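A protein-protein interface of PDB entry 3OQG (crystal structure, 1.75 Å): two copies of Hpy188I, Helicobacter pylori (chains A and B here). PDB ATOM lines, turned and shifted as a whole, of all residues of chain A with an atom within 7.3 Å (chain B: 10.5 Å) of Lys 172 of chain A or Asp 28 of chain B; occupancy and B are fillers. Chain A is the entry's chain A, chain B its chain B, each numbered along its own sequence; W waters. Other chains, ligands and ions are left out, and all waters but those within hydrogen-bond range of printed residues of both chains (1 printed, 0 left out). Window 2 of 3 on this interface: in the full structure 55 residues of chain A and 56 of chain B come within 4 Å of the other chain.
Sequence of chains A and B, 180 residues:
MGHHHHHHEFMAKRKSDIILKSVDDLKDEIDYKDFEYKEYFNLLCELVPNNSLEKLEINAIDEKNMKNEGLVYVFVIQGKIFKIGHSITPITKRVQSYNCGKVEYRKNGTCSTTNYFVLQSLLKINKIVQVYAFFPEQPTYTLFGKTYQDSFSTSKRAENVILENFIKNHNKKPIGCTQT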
ATOM      1  N   LEU A 163       8.383  -2.335  -2.774  1.00  0.00           N
ATOM      2  CA  LEU A 163       7.944  -3.634  -3.302  1.00  0.00           C
ATOM      3  C   LEU A 163       8.257  -4.777  -2.340  1.00  0.00           C
ATOM      4  O   LEU A 163       7.454  -5.699  -2.139  1.00  0.00           O
ATOM      5  CB  LEU A 163       8.597  -3.938  -4.654  1.00  0.00           C
ATOM      6  CG  LEU A 163       7.755  -3.804  -5.915  1.00  0.00           C
ATOM      7  CD1 LEU A 163       8.596  -4.257  -7.130  1.00  0.00           C
ATOM      8  CD2 LEU A 163       6.466  -4.620  -5.816  1.00  0.00           C
ATOM      9  N   ASN A 165       8.511  -4.438   0.851  1.00  0.00           N
ATOM     10  CA  ASN A 165       7.549  -4.223   1.945  1.00  0.00           C
ATOM     11  C   ASN A 165       6.154  -4.700   1.537  1.00  0.00           C
ATOM     12  O   ASN A 165       5.449  -5.337   2.320  1.00  0.00           O
ATOM     13  CB  ASN A 165       7.488  -2.743   2.352  1.00  0.00           C
ATOM     14  CG  ASN A 165       6.673  -2.507   3.626  1.00  0.00           C
ATOM     15  OD1 ASN A 165       7.102  -2.868   4.724  1.00  0.00           O
ATOM     16  ND2 ASN A 165       5.506  -1.894   3.485  1.00  0.00           N
ATOM     17  N   PHE A 166       5.770  -4.386   0.302  1.00  0.00           N
ATOM     18  CA  PHE A 166       4.485  -4.835  -0.267  1.00  0.00           C
ATOM     19  C   PHE A 166       4.352  -6.368  -0.182  1.00  0.00           C
ATOM     20  O   PHE A 166       3.328  -6.887   0.229  1.00  0.00           O
ATOM     21  CB  PHE A 166       4.402  -4.378  -1.726  1.00  0.00           C
ATOM     22  CG  PHE A 166       3.081  -4.635  -2.389  1.00  0.00           C
ATOM     23  CD1 PHE A 166       2.134  -3.625  -2.492  1.00  0.00           C
ATOM     24  CD2 PHE A 166       2.807  -5.860  -2.970  1.00  0.00           C
ATOM     25  CE1 PHE A 166       0.938  -3.841  -3.124  1.00  0.00           C
ATOM     26  CE2 PHE A 166       1.606  -6.081  -3.615  1.00  0.00           C
ATOM     27  CZ  PHE A 166       0.674  -5.065  -3.704  1.00  0.00           C
ATOM     28  N   ILE A 167       5.423  -7.067  -0.540  1.00  0.00           N
ATOM     29  CA  ILE A 167       5.446  -8.530  -0.559  1.00  0.00           C
ATOM     30  C   ILE A 167       5.281  -9.109   0.855  1.00  0.00           C
ATOM     31  O   ILE A 167       4.576 -10.106   1.059  1.00  0.00           O
ATOM     32  CB  ILE A 167       6.764  -9.035  -1.218  1.00  0.00           C
ATOM     33  CG1 ILE A 167       6.698  -8.836  -2.737  1.00  0.00           C
ATOM     34  CG2 ILE A 167       7.004 -10.502  -0.885  1.00  0.00           C
ATOM     35  CD1 ILE A 167       8.061  -8.796  -3.446  1.00  0.00           C
ATOM     36  N   LYS A 168       5.922  -8.482   1.834  1.00  0.00           N
ATOM     37  CA  LYS A 168       5.774  -8.891   3.227  1.00  0.00           C
ATOM     38  C   LYS A 168       4.359  -8.641   3.773  1.00  0.00           C
ATOM     39  O   LYS A 168       3.827  -9.418   4.561  1.00  0.00           O
ATOM     40  CB  LYS A 168       6.851  -8.204   4.080  1.00  0.00           C
ATOM     41  CG  LYS A 168       6.352  -7.404   5.231  1.00  0.00           C
ATOM     42  CD  LYS A 168       7.501  -6.810   6.013  1.00  0.00           C
ATOM     43  CE  LYS A 168       6.963  -5.855   7.068  1.00  0.00           C
ATOM     44  NZ  LYS A 168       6.259  -4.680   6.475  1.00  0.00           N
ATOM     45  N   ASN A 169       3.756  -7.541   3.341  1.00  0.00           N
ATOM     46  CA  ASN A 169       2.416  -7.197   3.779  1.00  0.00           C
ATOM     47  C   ASN A 169       1.324  -8.062   3.140  1.00  0.00           C
ATOM     48  O   ASN A 169       0.393  -8.482   3.830  1.00  0.00           O
ATOM     49  CB  ASN A 169       2.148  -5.715   3.507  1.00  0.00           C
ATOM     50  CG  ASN A 169       3.069  -4.801   4.305  1.00  0.00           C
ATOM     51  OD1 ASN A 169       3.709  -5.237   5.271  1.00  0.00           O
ATOM     52  ND2 ASN A 169       3.124  -3.519   3.922  1.00  0.00           N
ATOM     53  N   HIS A 170       1.459  -8.350   1.847  1.00  0.00           N
ATOM     54  CA  HIS A 170       0.403  -9.000   1.066  1.00  0.00           C
ATOM     55  C   HIS A 170       0.790 -10.358   0.489  1.00  0.00           C
ATOM     56  O   HIS A 170      -0.041 -11.032  -0.119  1.00  0.00           O
ATOM     57  CB  HIS A 170      -0.022  -8.062  -0.077  1.00  0.00           C
ATOM     58  CG  HIS A 170      -0.382  -6.690   0.392  1.00  0.00           C
ATOM     59  ND1 HIS A 170      -1.468  -6.448   1.202  1.00  0.00           N
ATOM     60  CD2 HIS A 170       0.197  -5.485   0.168  1.00  0.00           C
ATOM     61  CE1 HIS A 170      -1.535  -5.158   1.472  1.00  0.00           C
ATOM     62  NE2 HIS A 170      -0.534  -4.552   0.858  1.00  0.00           N
ATOM     63  N   ASN A 171       2.039 -10.761   0.678  1.00  0.00           N
ATOM     64  CA  ASN A 171       2.513 -12.055   0.190  1.00  0.00           C
ATOM     65  C   ASN A 171       2.325 -12.273  -1.307  1.00  0.00           C
ATOM     66  O   ASN A 171       2.052 -13.389  -1.760  1.00  0.00           O
ATOM     67  CB  ASN A 171       1.840 -13.195   0.956  1.00  0.00           C
ATOM     68  CG  ASN A 171       2.622 -14.466   0.866  1.00  0.00           C
ATOM     69  OD1 ASN A 171       3.817 -14.432   0.563  1.00  0.00           O
ATOM     70  ND2 ASN A 171       1.974 -15.598   1.114  1.00  0.00           N
ATOM     71  N   LYS A 172       2.484 -11.203  -2.075  1.00  0.00           N
ATOM     72  CA  LYS A 172       2.485 -11.294  -3.526  1.00  0.00           C
ATOM     73  C   LYS A 172       3.005  -9.964  -4.051  1.00  0.00           C
ATOM     74  O   LYS A 172       3.081  -8.985  -3.290  1.00  0.00           O
ATOM     75  CB  LYS A 172       1.073 -11.545  -4.067  1.00  0.00           C
ATOM     76  CG  LYS A 172       0.048 -10.544  -3.586  1.00  0.00           C
ATOM     77  CD  LYS A 172      -1.065 -10.287  -4.594  1.00  0.00           C
ATOM     78  CE  LYS A 172      -2.111 -11.372  -4.576  1.00  0.00           C
ATOM     79  NZ  LYS A 172      -2.672 -11.566  -5.953  1.00  0.00           N
ATOM     80  N   LYS A 173       3.382  -9.949  -5.333  1.00  0.00           N
ATOM     81  CA  LYS A 173       3.671  -8.714  -6.063  1.00  0.00           C
ATOM     82  C   LYS A 173       2.454  -8.388  -6.900  1.00  0.00           C
ATOM     83  O   LYS A 173       1.659  -9.272  -7.196  1.00  0.00           O
ATOM     84  CB  LYS A 173       4.847  -8.895  -7.027  1.00  0.00           C
ATOM     85  CG  LYS A 173       6.221  -8.959  -6.388  1.00  0.00           C
ATOM     86  CD  LYS A 173       7.313  -9.124  -7.456  1.00  0.00           C
ATOM     87  CE  LYS A 173       7.460 -10.592  -7.892  1.00  0.00           C
ATOM     88  NZ  LYS A 173       6.349 -11.079  -8.793  1.00  0.00           N
ATOM     89  N   PRO A 174       2.297  -7.111  -7.299  1.00  0.00           N
ATOM     90  CA  PRO A 174       1.211  -6.816  -8.224  1.00  0.00           C
ATOM     91  C   PRO A 174       1.320  -7.637  -9.505  1.00  0.00           C
ATOM     92  O   PRO A 174       2.422  -7.939  -9.957  1.00  0.00           O
ATOM     93  CB  PRO A 174       1.415  -5.336  -8.538  1.00  0.00           C
ATOM     94  CG  PRO A 174       2.151  -4.800  -7.336  1.00  0.00           C
ATOM     95  CD  PRO A 174       3.040  -5.905  -6.910  1.00  0.00           C
ATOM     96  N   ILE A 175       0.176  -7.983 -10.081  1.00  0.00           N
ATOM     97  CA  ILE A 175       0.124  -8.763 -11.306  1.00  0.00           C
ATOM     98  C   ILE A 175       0.974  -8.213 -12.463  1.00  0.00           C
ATOM     99  O   ILE A 175       1.565  -8.983 -13.246  1.00  0.00           O
ATOM    100  CB  ILE A 175      -1.349  -8.971 -11.754  1.00  0.00           C
ATOM    101  CG1 ILE A 175      -1.438 -10.046 -12.840  1.00  0.00           C
ATOM    102  CG2 ILE A 175      -2.016  -7.651 -12.204  1.00  0.00           C
ATOM    103  CD1 ILE A 175      -2.805 -10.708 -12.869  1.00  0.00           C
ATOM    104  N   LYS B  15       5.889 -15.064 -19.172  1.00  0.00           N
ATOM    105  CA  LYS B  15       4.778 -14.345 -18.561  1.00  0.00           C
ATOM    106  C   LYS B  15       4.307 -13.161 -19.407  1.00  0.00           C
ATOM    107  O   LYS B  15       3.105 -12.938 -19.557  1.00  0.00           O
ATOM    108  CB  LYS B  15       5.145 -13.856 -17.150  1.00  0.00           C
ATOM    109  CG  LYS B  15       3.977 -13.159 -16.450  1.00  0.00           C
ATOM    110  CD  LYS B  15       3.922 -13.411 -14.944  1.00  0.00           C
ATOM    111  CE  LYS B  15       4.696 -12.390 -14.153  1.00  0.00           C
ATOM    112  NZ  LYS B  15       4.382 -12.450 -12.707  1.00  0.00           N
ATOM    113  N   LEU B  20      -3.392  -9.433 -20.206  1.00  0.00           N
ATOM    114  CA  LEU B  20      -4.631  -9.427 -19.428  1.00  0.00           C
ATOM    115  C   LEU B  20      -5.798  -9.047 -20.343  1.00  0.00           C
ATOM    116  O   LEU B  20      -5.642  -8.222 -21.248  1.00  0.00           O
ATOM    117  CB  LEU B  20      -4.530  -8.477 -18.245  1.00  0.00           C
ATOM    118  CG  LEU B  20      -3.395  -8.712 -17.246  1.00  0.00           C
ATOM    119  CD1 LEU B  20      -3.622  -7.863 -15.998  1.00  0.00           C
ATOM    120  CD2 LEU B  20      -3.269 -10.174 -16.876  1.00  0.00           C
ATOM    121  N   SER B  22      -9.321  -8.403 -19.166  1.00  0.00           N
ATOM    122  CA  SER B  22     -10.348  -7.530 -18.611  1.00  0.00           C
ATOM    123  C   SER B  22     -10.065  -7.172 -17.170  1.00  0.00           C
ATOM    124  O   SER B  22      -9.163  -7.730 -16.547  1.00  0.00           O
ATOM    125  CB  SER B  22     -11.715  -8.201 -18.687  1.00  0.00           C
ATOM    126  OG  SER B  22     -11.921  -9.021 -17.561  1.00  0.00           O
ATOM    127  N   VAL B  23     -10.860  -6.257 -16.633  1.00  0.00           N
ATOM    128  CA  VAL B  23     -10.714  -5.843 -15.246  1.00  0.00           C
ATOM    129  C   VAL B  23     -10.927  -7.036 -14.302  1.00  0.00           C
ATOM    130  O   VAL B  23     -10.457  -7.029 -13.167  1.00  0.00           O
ATOM    131  CB  VAL B  23     -11.684  -4.678 -14.898  1.00  0.00           C
ATOM    132  CG1 VAL B  23     -13.088  -5.205 -14.636  1.00  0.00           C
ATOM    133  CG2 VAL B  23     -11.159  -3.887 -13.705  1.00  0.00           C
ATOM    134  N   ASP B  24     -11.626  -8.064 -14.780  1.00  0.00           N
ATOM    135  CA  ASP B  24     -11.833  -9.290 -13.989  1.00  0.00           C
ATOM    136  C   ASP B  24     -10.510  -9.988 -13.661  1.00  0.00           C
ATOM    137  O   ASP B  24     -10.413 -10.700 -12.661  1.00  0.00           O
ATOM    138  CB  ASP B  24     -12.756 -10.272 -14.721  1.00  0.00           C
ATOM    139  CG  ASP B  24     -14.184  -9.768 -14.844  1.00  0.00           C
ATOM    140  OD1 ASP B  24     -14.549  -8.772 -14.184  1.00  0.00           O
ATOM    141  OD2 ASP B  24     -14.950 -10.384 -15.614  1.00  0.00           O
ATOM    142  N   ASP B  25      -9.493  -9.777 -14.499  1.00  0.00           N
ATOM    143  CA  ASP B  25      -8.152 -10.309 -14.236  1.00  0.00           C
ATOM    144  C   ASP B  25      -7.475  -9.658 -13.033  1.00  0.00           C
ATOM    145  O   ASP B  25      -6.489 -10.185 -12.542  1.00  0.00           O
ATOM    146  CB  ASP B  25      -7.264 -10.156 -15.467  1.00  0.00           C
ATOM    147  CG  ASP B  25      -7.646 -11.103 -16.583  1.00  0.00           C
ATOM    148  OD1 ASP B  25      -8.349 -12.102 -16.324  1.00  0.00           O
ATOM    149  OD2 ASP B  25      -7.219 -10.865 -17.728  1.00  0.00           O
ATOM    150  N   LEU B  26      -8.010  -8.535 -12.552  1.00  0.00           N
ATOM    151  CA  LEU B  26      -7.465  -7.856 -11.386  1.00  0.00           C
ATOM    152  C   LEU B  26      -8.183  -8.194 -10.072  1.00  0.00           C
ATOM    153  O   LEU B  26      -7.866  -7.607  -9.040  1.00  0.00           O
ATOM    154  CB  LEU B  26      -7.511  -6.337 -11.605  1.00  0.00           C
ATOM    155  CG  LEU B  26      -6.860  -5.805 -12.888  1.00  0.00           C
ATOM    156  CD1 LEU B  26      -7.117  -4.320 -13.054  1.00  0.00           C
ATOM    157  CD2 LEU B  26      -5.364  -6.126 -12.885  1.00  0.00           C
ATOM    158  N   LYS B  27      -9.150  -9.109 -10.122  1.00  0.00           N
ATOM    159  CA  LYS B  27     -10.033  -9.395  -8.987  1.00  0.00           C
ATOM    160  C   LYS B  27      -9.293  -9.820  -7.702  1.00  0.00           C
ATOM    161  O   LYS B  27      -9.764  -9.528  -6.603  1.00  0.00           O
ATOM    162  CB  LYS B  27     -11.063 -10.471  -9.365  1.00  0.00           C
ATOM    163  CG  LYS B  27     -10.460 -11.853  -9.584  1.00  0.00           C
ATOM    164  CD  LYS B  27     -11.514 -12.889 -10.012  1.00  0.00           C
ATOM    165  CE  LYS B  27     -10.879 -13.966 -10.879  1.00  0.00           C
ATOM    166  NZ  LYS B  27     -10.219 -13.364 -12.092  1.00  0.00           N
ATOM    167  N   ASP B  28      -8.137 -10.464  -7.847  1.00  0.00           N
ATOM    168  CA  ASP B  28      -7.332 -10.913  -6.691  1.00  0.00           C
ATOM    169  C   ASP B  28      -6.186  -9.978  -6.342  1.00  0.00           C
ATOM    170  O   ASP B  28      -5.361 -10.297  -5.470  1.00  0.00           O
ATOM    171  CB  ASP B  28      -6.743 -12.303  -6.957  1.00  0.00           C
ATOM    172  CG  ASP B  28      -7.804 -13.375  -7.143  1.00  0.00           C
ATOM    173  OD1 ASP B  28      -8.894 -13.268  -6.558  1.00  0.00           O
ATOM    174  OD2 ASP B  28      -7.517 -14.342  -7.880  1.00  0.00           O
ATOM    175  N   GLU B  29      -6.117  -8.834  -7.017  1.00  0.00           N
ATOM    176  CA  GLU B  29      -5.099  -7.851  -6.709  1.00  0.00           C
ATOM    177  C   GLU B  29      -5.398  -7.121  -5.408  1.00  0.00           C
ATOM    178  O   GLU B  29      -6.469  -7.283  -4.809  1.00  0.00           O
ATOM    179  CB  GLU B  29      -4.899  -6.880  -7.893  1.00  0.00           C
ATOM    180  CG  GLU B  29      -4.413  -7.586  -9.165  1.00  0.00           C
ATOM    181  CD  GLU B  29      -3.255  -8.537  -8.900  1.00  0.00           C
ATOM    182  OE1 GLU B  29      -2.180  -8.060  -8.476  1.00  0.00           O
ATOM    183  OE2 GLU B  29      -3.427  -9.775  -9.054  1.00  0.00           O
ATOM    184  N   ILE B  30      -4.406  -6.382  -4.945  1.00  0.00           N
ATOM    185  CA  ILE B  30      -4.451  -5.650  -3.685  1.00  0.00           C
ATOM    186  C   ILE B  30      -5.105  -4.290  -3.934  1.00  0.00           C
ATOM    187  O   ILE B  30      -4.774  -3.612  -4.895  1.00  0.00           O
ATOM    188  CB  ILE B  30      -3.010  -5.441  -3.137  1.00  0.00           C
ATOM    189  CG1 ILE B  30      -2.331  -6.787  -2.860  1.00  0.00           C
ATOM    190  CG2 ILE B  30      -2.995  -4.547  -1.872  1.00  0.00           C
ATOM    191  CD1 ILE B  30      -3.189  -7.794  -2.081  1.00  0.00           C
ATOM    192  N   ASP B  31      -6.034  -3.895  -3.063  1.00  0.00           N
ATOM    193  CA  ASP B  31      -6.634  -2.568  -3.154  1.00  0.00           C
ATOM    194  C   ASP B  31      -5.636  -1.482  -2.814  1.00  0.00           C
ATOM    195  O   ASP B  31      -4.853  -1.619  -1.880  1.00  0.00           O
ATOM    196  CB  ASP B  31      -7.809  -2.425  -2.183  1.00  0.00           C
ATOM    197  CG  ASP B  31      -8.985  -3.304  -2.537  1.00  0.00           C
ATOM    198  OD1 ASP B  31      -9.164  -3.670  -3.712  1.00  0.00           O
ATOM    199  OD2 ASP B  31      -9.764  -3.610  -1.609  1.00  0.00           O
ATOM    200  N   TYR B  32      -5.707  -0.370  -3.549  1.00  0.00           N
ATOM    201  CA  TYR B  32      -4.828   0.746  -3.308  1.00  0.00           C
ATOM    202  C   TYR B  32      -5.033   1.262  -1.876  1.00  0.00           C
ATOM    203  O   TYR B  32      -4.088   1.702  -1.243  1.00  0.00           O
ATOM    204  CB  TYR B  32      -5.038   1.860  -4.361  1.00  0.00           C
ATOM    205  CG  TYR B  32      -4.103   3.015  -4.147  1.00  0.00           C
ATOM    206  CD1 TYR B  32      -2.758   2.906  -4.488  1.00  0.00           C
ATOM    207  CD2 TYR B  32      -4.547   4.212  -3.579  1.00  0.00           C
ATOM    208  CE1 TYR B  32      -1.874   3.962  -4.274  1.00  0.00           C
ATOM    209  CE2 TYR B  32      -3.676   5.279  -3.359  1.00  0.00           C
ATOM    210  CZ  TYR B  32      -2.339   5.149  -3.698  1.00  0.00           C
ATOM    211  OH  TYR B  32      -1.459   6.188  -3.480  1.00  0.00           O
ATOM    212  N   ASP B  34      -5.223  -0.375   0.697  1.00  0.00           N
ATOM    213  CA  ASP B  34      -4.384  -1.225   1.561  1.00  0.00           C
ATOM    214  C   ASP B  34      -2.867  -1.122   1.335  1.00  0.00           C
ATOM    215  O   ASP B  34      -2.093  -1.884   1.905  1.00  0.00           O
ATOM    216  CB  ASP B  34      -4.831  -2.677   1.406  1.00  0.00           C
ATOM    217  CG  ASP B  34      -6.260  -2.886   1.838  1.00  0.00           C
ATOM    218  OD1 ASP B  34      -6.728  -2.166   2.752  1.00  0.00           O
ATOM    219  OD2 ASP B  34      -6.936  -3.758   1.264  1.00  0.00           O
ATOM    220  N   PHE B  35      -2.449  -0.151   0.527  1.00  0.00           N
ATOM    221  CA  PHE B  35      -1.050   0.143   0.267  1.00  0.00           C
ATOM    222  C   PHE B  35      -0.450   0.961   1.424  1.00  0.00           C
ATOM    223  O   PHE B  35      -0.906   2.069   1.687  1.00  0.00           O
ATOM    224  CB  PHE B  35      -0.994   0.919  -1.055  1.00  0.00           C
ATOM    225  CG  PHE B  35       0.382   1.310  -1.505  1.00  0.00           C
ATOM    226  CD1 PHE B  35       1.439   0.419  -1.468  1.00  0.00           C
ATOM    227  CD2 PHE B  35       0.598   2.573  -2.050  1.00  0.00           C
ATOM    228  CE1 PHE B  35       2.694   0.799  -1.928  1.00  0.00           C
ATOM    229  CE2 PHE B  35       1.838   2.953  -2.482  1.00  0.00           C
ATOM    230  CZ  PHE B  35       2.893   2.063  -2.432  1.00  0.00           C
ATOM    231  N   ILE B  77      -6.319   0.502 -11.218  1.00  0.00           N
ATOM    232  CA  ILE B  77      -7.518   0.359 -12.030  1.00  0.00           C
ATOM    233  C   ILE B  77      -8.667  -0.084 -11.141  1.00  0.00           C
ATOM    234  O   ILE B  77      -8.605  -1.158 -10.535  1.00  0.00           O
ATOM    235  CB  ILE B  77      -7.325  -0.635 -13.184  1.00  0.00           C
ATOM    236  CG1 ILE B  77      -6.114  -0.223 -14.045  1.00  0.00           C
ATOM    237  CG2 ILE B  77      -8.629  -0.791 -14.007  1.00  0.00           C
ATOM    238  CD1 ILE B  77      -5.719  -1.255 -15.095  1.00  0.00           C
ATOM    239  N   GLN B  78      -9.722   0.731 -11.081  1.00  0.00           N
ATOM    240  CA  GLN B  78     -10.856   0.449 -10.223  1.00  0.00           C
ATOM    241  C   GLN B  78     -10.439   0.044  -8.808  1.00  0.00           C
ATOM    242  O   GLN B  78     -10.922  -0.962  -8.272  1.00  0.00           O
ATOM    243  CB  GLN B  78     -11.723  -0.661 -10.836  1.00  0.00           C
ATOM    244  CG  GLN B  78     -12.391  -0.288 -12.132  1.00  0.00           C
ATOM    245  CD  GLN B  78     -13.449  -1.282 -12.574  1.00  0.00           C
ATOM    246  OE1 GLN B  78     -13.719  -2.286 -11.896  1.00  0.00           O
ATOM    247  NE2 GLN B  78     -14.027  -1.032 -13.724  1.00  0.00           N
ATOM    248  N   GLY B  79      -9.551   0.820  -8.204  1.00  0.00           N
ATOM    249  CA  GLY B  79      -9.141   0.603  -6.825  1.00  0.00           C
ATOM    250  C   GLY B  79      -8.103  -0.478  -6.613  1.00  0.00           C
ATOM    251  O   GLY B  79      -7.631  -0.642  -5.488  1.00  0.00           O
ATOM    252  N   LYS B  80      -7.739  -1.194  -7.681  1.00  0.00           N
ATOM    253  CA  LYS B  80      -6.783  -2.331  -7.594  1.00  0.00           C
ATOM    254  C   LYS B  80      -5.420  -1.918  -8.131  1.00  0.00           C
ATOM    255  O   LYS B  80      -5.313  -1.287  -9.183  1.00  0.00           O
ATOM    256  CB  LYS B  80      -7.259  -3.511  -8.431  1.00  0.00           C
ATOM    257  CG  LYS B  80      -8.518  -4.205  -7.938  1.00  0.00           C
ATOM    258  CD  LYS B  80      -8.332  -4.782  -6.552  1.00  0.00           C
ATOM    259  CE  LYS B  80      -9.417  -5.799  -6.223  1.00  0.00           C
ATOM    260  NZ  LYS B  80      -9.250  -6.275  -4.837  1.00  0.00           N
ATOM    261  N   ILE B  81      -4.375  -2.329  -7.432  1.00  0.00           N
ATOM    262  CA  ILE B  81      -3.006  -2.056  -7.855  1.00  0.00           C
ATOM    263  C   ILE B  81      -2.614  -3.035  -8.972  1.00  0.00           C
ATOM    264  O   ILE B  81      -2.543  -4.258  -8.756  1.00  0.00           O
ATOM    265  CB  ILE B  81      -2.019  -2.157  -6.670  1.00  0.00           C
ATOM    266  CG1 ILE B  81      -2.352  -1.078  -5.614  1.00  0.00           C
ATOM    267  CG2 ILE B  81      -0.568  -2.047  -7.182  1.00  0.00           C
ATOM    268  CD1 ILE B  81      -1.503  -1.149  -4.320  1.00  0.00           C
ATOM    269  N   PHE B  82      -2.409  -2.476 -10.167  1.00  0.00           N
ATOM    270  CA  PHE B  82      -1.973  -3.228 -11.337  1.00  0.00           C
ATOM    271  C   PHE B  82      -0.435  -3.375 -11.355  1.00  0.00           C
ATOM    272  O   PHE B  82       0.104  -4.457 -11.609  1.00  0.00           O
ATOM    273  CB  PHE B  82      -2.481  -2.558 -12.619  1.00  0.00           C
ATOM    274  CG  PHE B  82      -1.813  -3.060 -13.872  1.00  0.00           C
ATOM    275  CD1 PHE B  82      -2.167  -4.271 -14.425  1.00  0.00           C
ATOM    276  CD2 PHE B  82      -0.797  -2.330 -14.466  1.00  0.00           C
ATOM    277  CE1 PHE B  82      -1.529  -4.742 -15.569  1.00  0.00           C
ATOM    278  CE2 PHE B  82      -0.154  -2.812 -15.610  1.00  0.00           C
ATOM    279  CZ  PHE B  82      -0.534  -4.003 -16.159  1.00  0.00           C
ATOM    280  N   LYS B  83       0.276  -2.289 -11.081  1.00  0.00           N
ATOM    281  CA  LYS B  83       1.721  -2.366 -10.968  1.00  0.00           C
ATOM    282  C   LYS B  83       2.307  -1.212 -10.199  1.00  0.00           C
ATOM    283  O   LYS B  83       1.661  -0.194 -10.002  1.00  0.00           O
ATOM    284  CB  LYS B  83       2.395  -2.489 -12.341  1.00  0.00           C
ATOM    285  CG  LYS B  83       2.769  -1.237 -13.042  1.00  0.00           C
ATOM    286  CD  LYS B  83       3.699  -1.550 -14.242  1.00  0.00           C
ATOM    287  CE  LYS B  83       5.204  -1.487 -13.927  1.00  0.00           C
ATOM    288  NZ  LYS B  83       6.048  -1.713 -15.138  1.00  0.00           N
ATOM    289  N   ILE B  84       3.540  -1.437  -9.752  1.00  0.00           N
ATOM    290  CA  ILE B  84       4.376  -0.429  -9.130  1.00  0.00           C
ATOM    291  C   ILE B  84       5.648  -0.379  -9.983  1.00  0.00           C
ATOM    292  O   ILE B  84       6.210  -1.417 -10.335  1.00  0.00           O
ATOM    293  CB  ILE B  84       4.719  -0.772  -7.674  1.00  0.00           C
ATOM    294  CG1 ILE B  84       3.453  -0.844  -6.792  1.00  0.00           C
ATOM    295  CG2 ILE B  84       5.712   0.244  -7.103  1.00  0.00           C
ATOM    296  CD1 ILE B  84       3.698  -1.516  -5.414  1.00  0.00           C
HETATM  297  O   HOH W   1       3.165 -10.743 -10.373  1.00  0.00           O
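Of chain B, only Ile 30 (3.6 Å), Ile 81 (3.8 Å) and Ile 84 (3.9 Å) come within 4 Å of Phe 166 of chain A. No residue of chain B comes within 4 Å of Ile 167 of chain A. Of the printed residues of chain B, His 170 of chain A touches Ile 30 (3.7 Å) and Asp 34 (3.3 Å). No residue of chain B comes within 4 Å of Asn 171 of chain A. Of the printed residues of chain B, Ile 175 of chain A touches Asp 25, Leu 26, Glu 29 and Phe 82. Asp 28 of chain B touches just one residue of chain A: Lys 172 (3.0 Å). Printed residues of chain A within 4 Å of Glu 29 of chain B: Lys 172, Pro 174 and Ile 175. Printed residues of chain A within 4 Å of Ile 84 of chain B: Phe 166.
The backbone carbonyl oxygen (O) of Ile 30 of chain B lies within hydrogen-bond range of the backbone NH (N) of Ile 81 of chain B, 2.9 Å away. The backbone carbonyl oxygen (O) of Glu 29 of chain B lies within hydrogen-bond range of the side-chain amino group (NZ) of Lys 80 of chain B (3.0 Å).
No position is printed for both chains. Of the 15 pairs that touch across the chains among the printed residues, none has its exchanged pair printed and touching as well.
Among the printed residues, merely in contact across the chains: Pro 174 of chain A with Phe 82 of chain B (3.5 Å), Phe 166 of chain A with Ile 30 of chain B (3.6 Å), Pro 174 of chain A with Glu 29 of chain B (3.6 Å), His 170 of chain A with Ile 30 of chain B (3.7 Å), Ile 175 of chain A with Asp 25 of chain B (3.7 Å), Ile 175 of chain A with Leu 26 of chain B (3.7 Å), Phe 166 of chain A with Ile 81 of chain B (3.8 Å), Ile 175 of chain A with Phe 82 of chain B (3.8 Å), Pro 174 of chain A with Lys 83 of chain B (3.8 Å), Pro 174 of chain A with Ile 81 of chain B (3.9 Å) and Phe 166 of chain A with Ile 84 of chain B (3.9 Å).
Of the 23 printed residues of chain B, 10 touch a printed residue of chain A. Among the printed residues, Asp or Glu carboxylates within 4 Å of a Lys or Arg side-chain nitrogen of the other chain: Lys 172 of chain A with Glu 29 of chain B (3.7 Å).
The side-chain amino group of Lys 172 of chain A lies within hydrogen-bond range of the backbone carbonyl oxygen of Asp 28 of chain B. OE1 of Glu 29 of chain B is in hydrogen-bond range of N of Ile 175 of chain A (2.9 Å). NZ of Lys 172 of chain A lies within salt-bridge range of OE2 of Glu 29 of chain B, at 3.7 Å. A ring nitrogen (NE2) of His 170 of chain A lies within hydrogen-bond range of the backbone carbonyl oxygen (O) of Asp 34 of chain B (3.3 Å).
Water W1 lies within hydrogen-bond range of O of Pro 174 of chain A (2.9 Å) and NZ of Lys 15 of chain B (3.1 Å).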
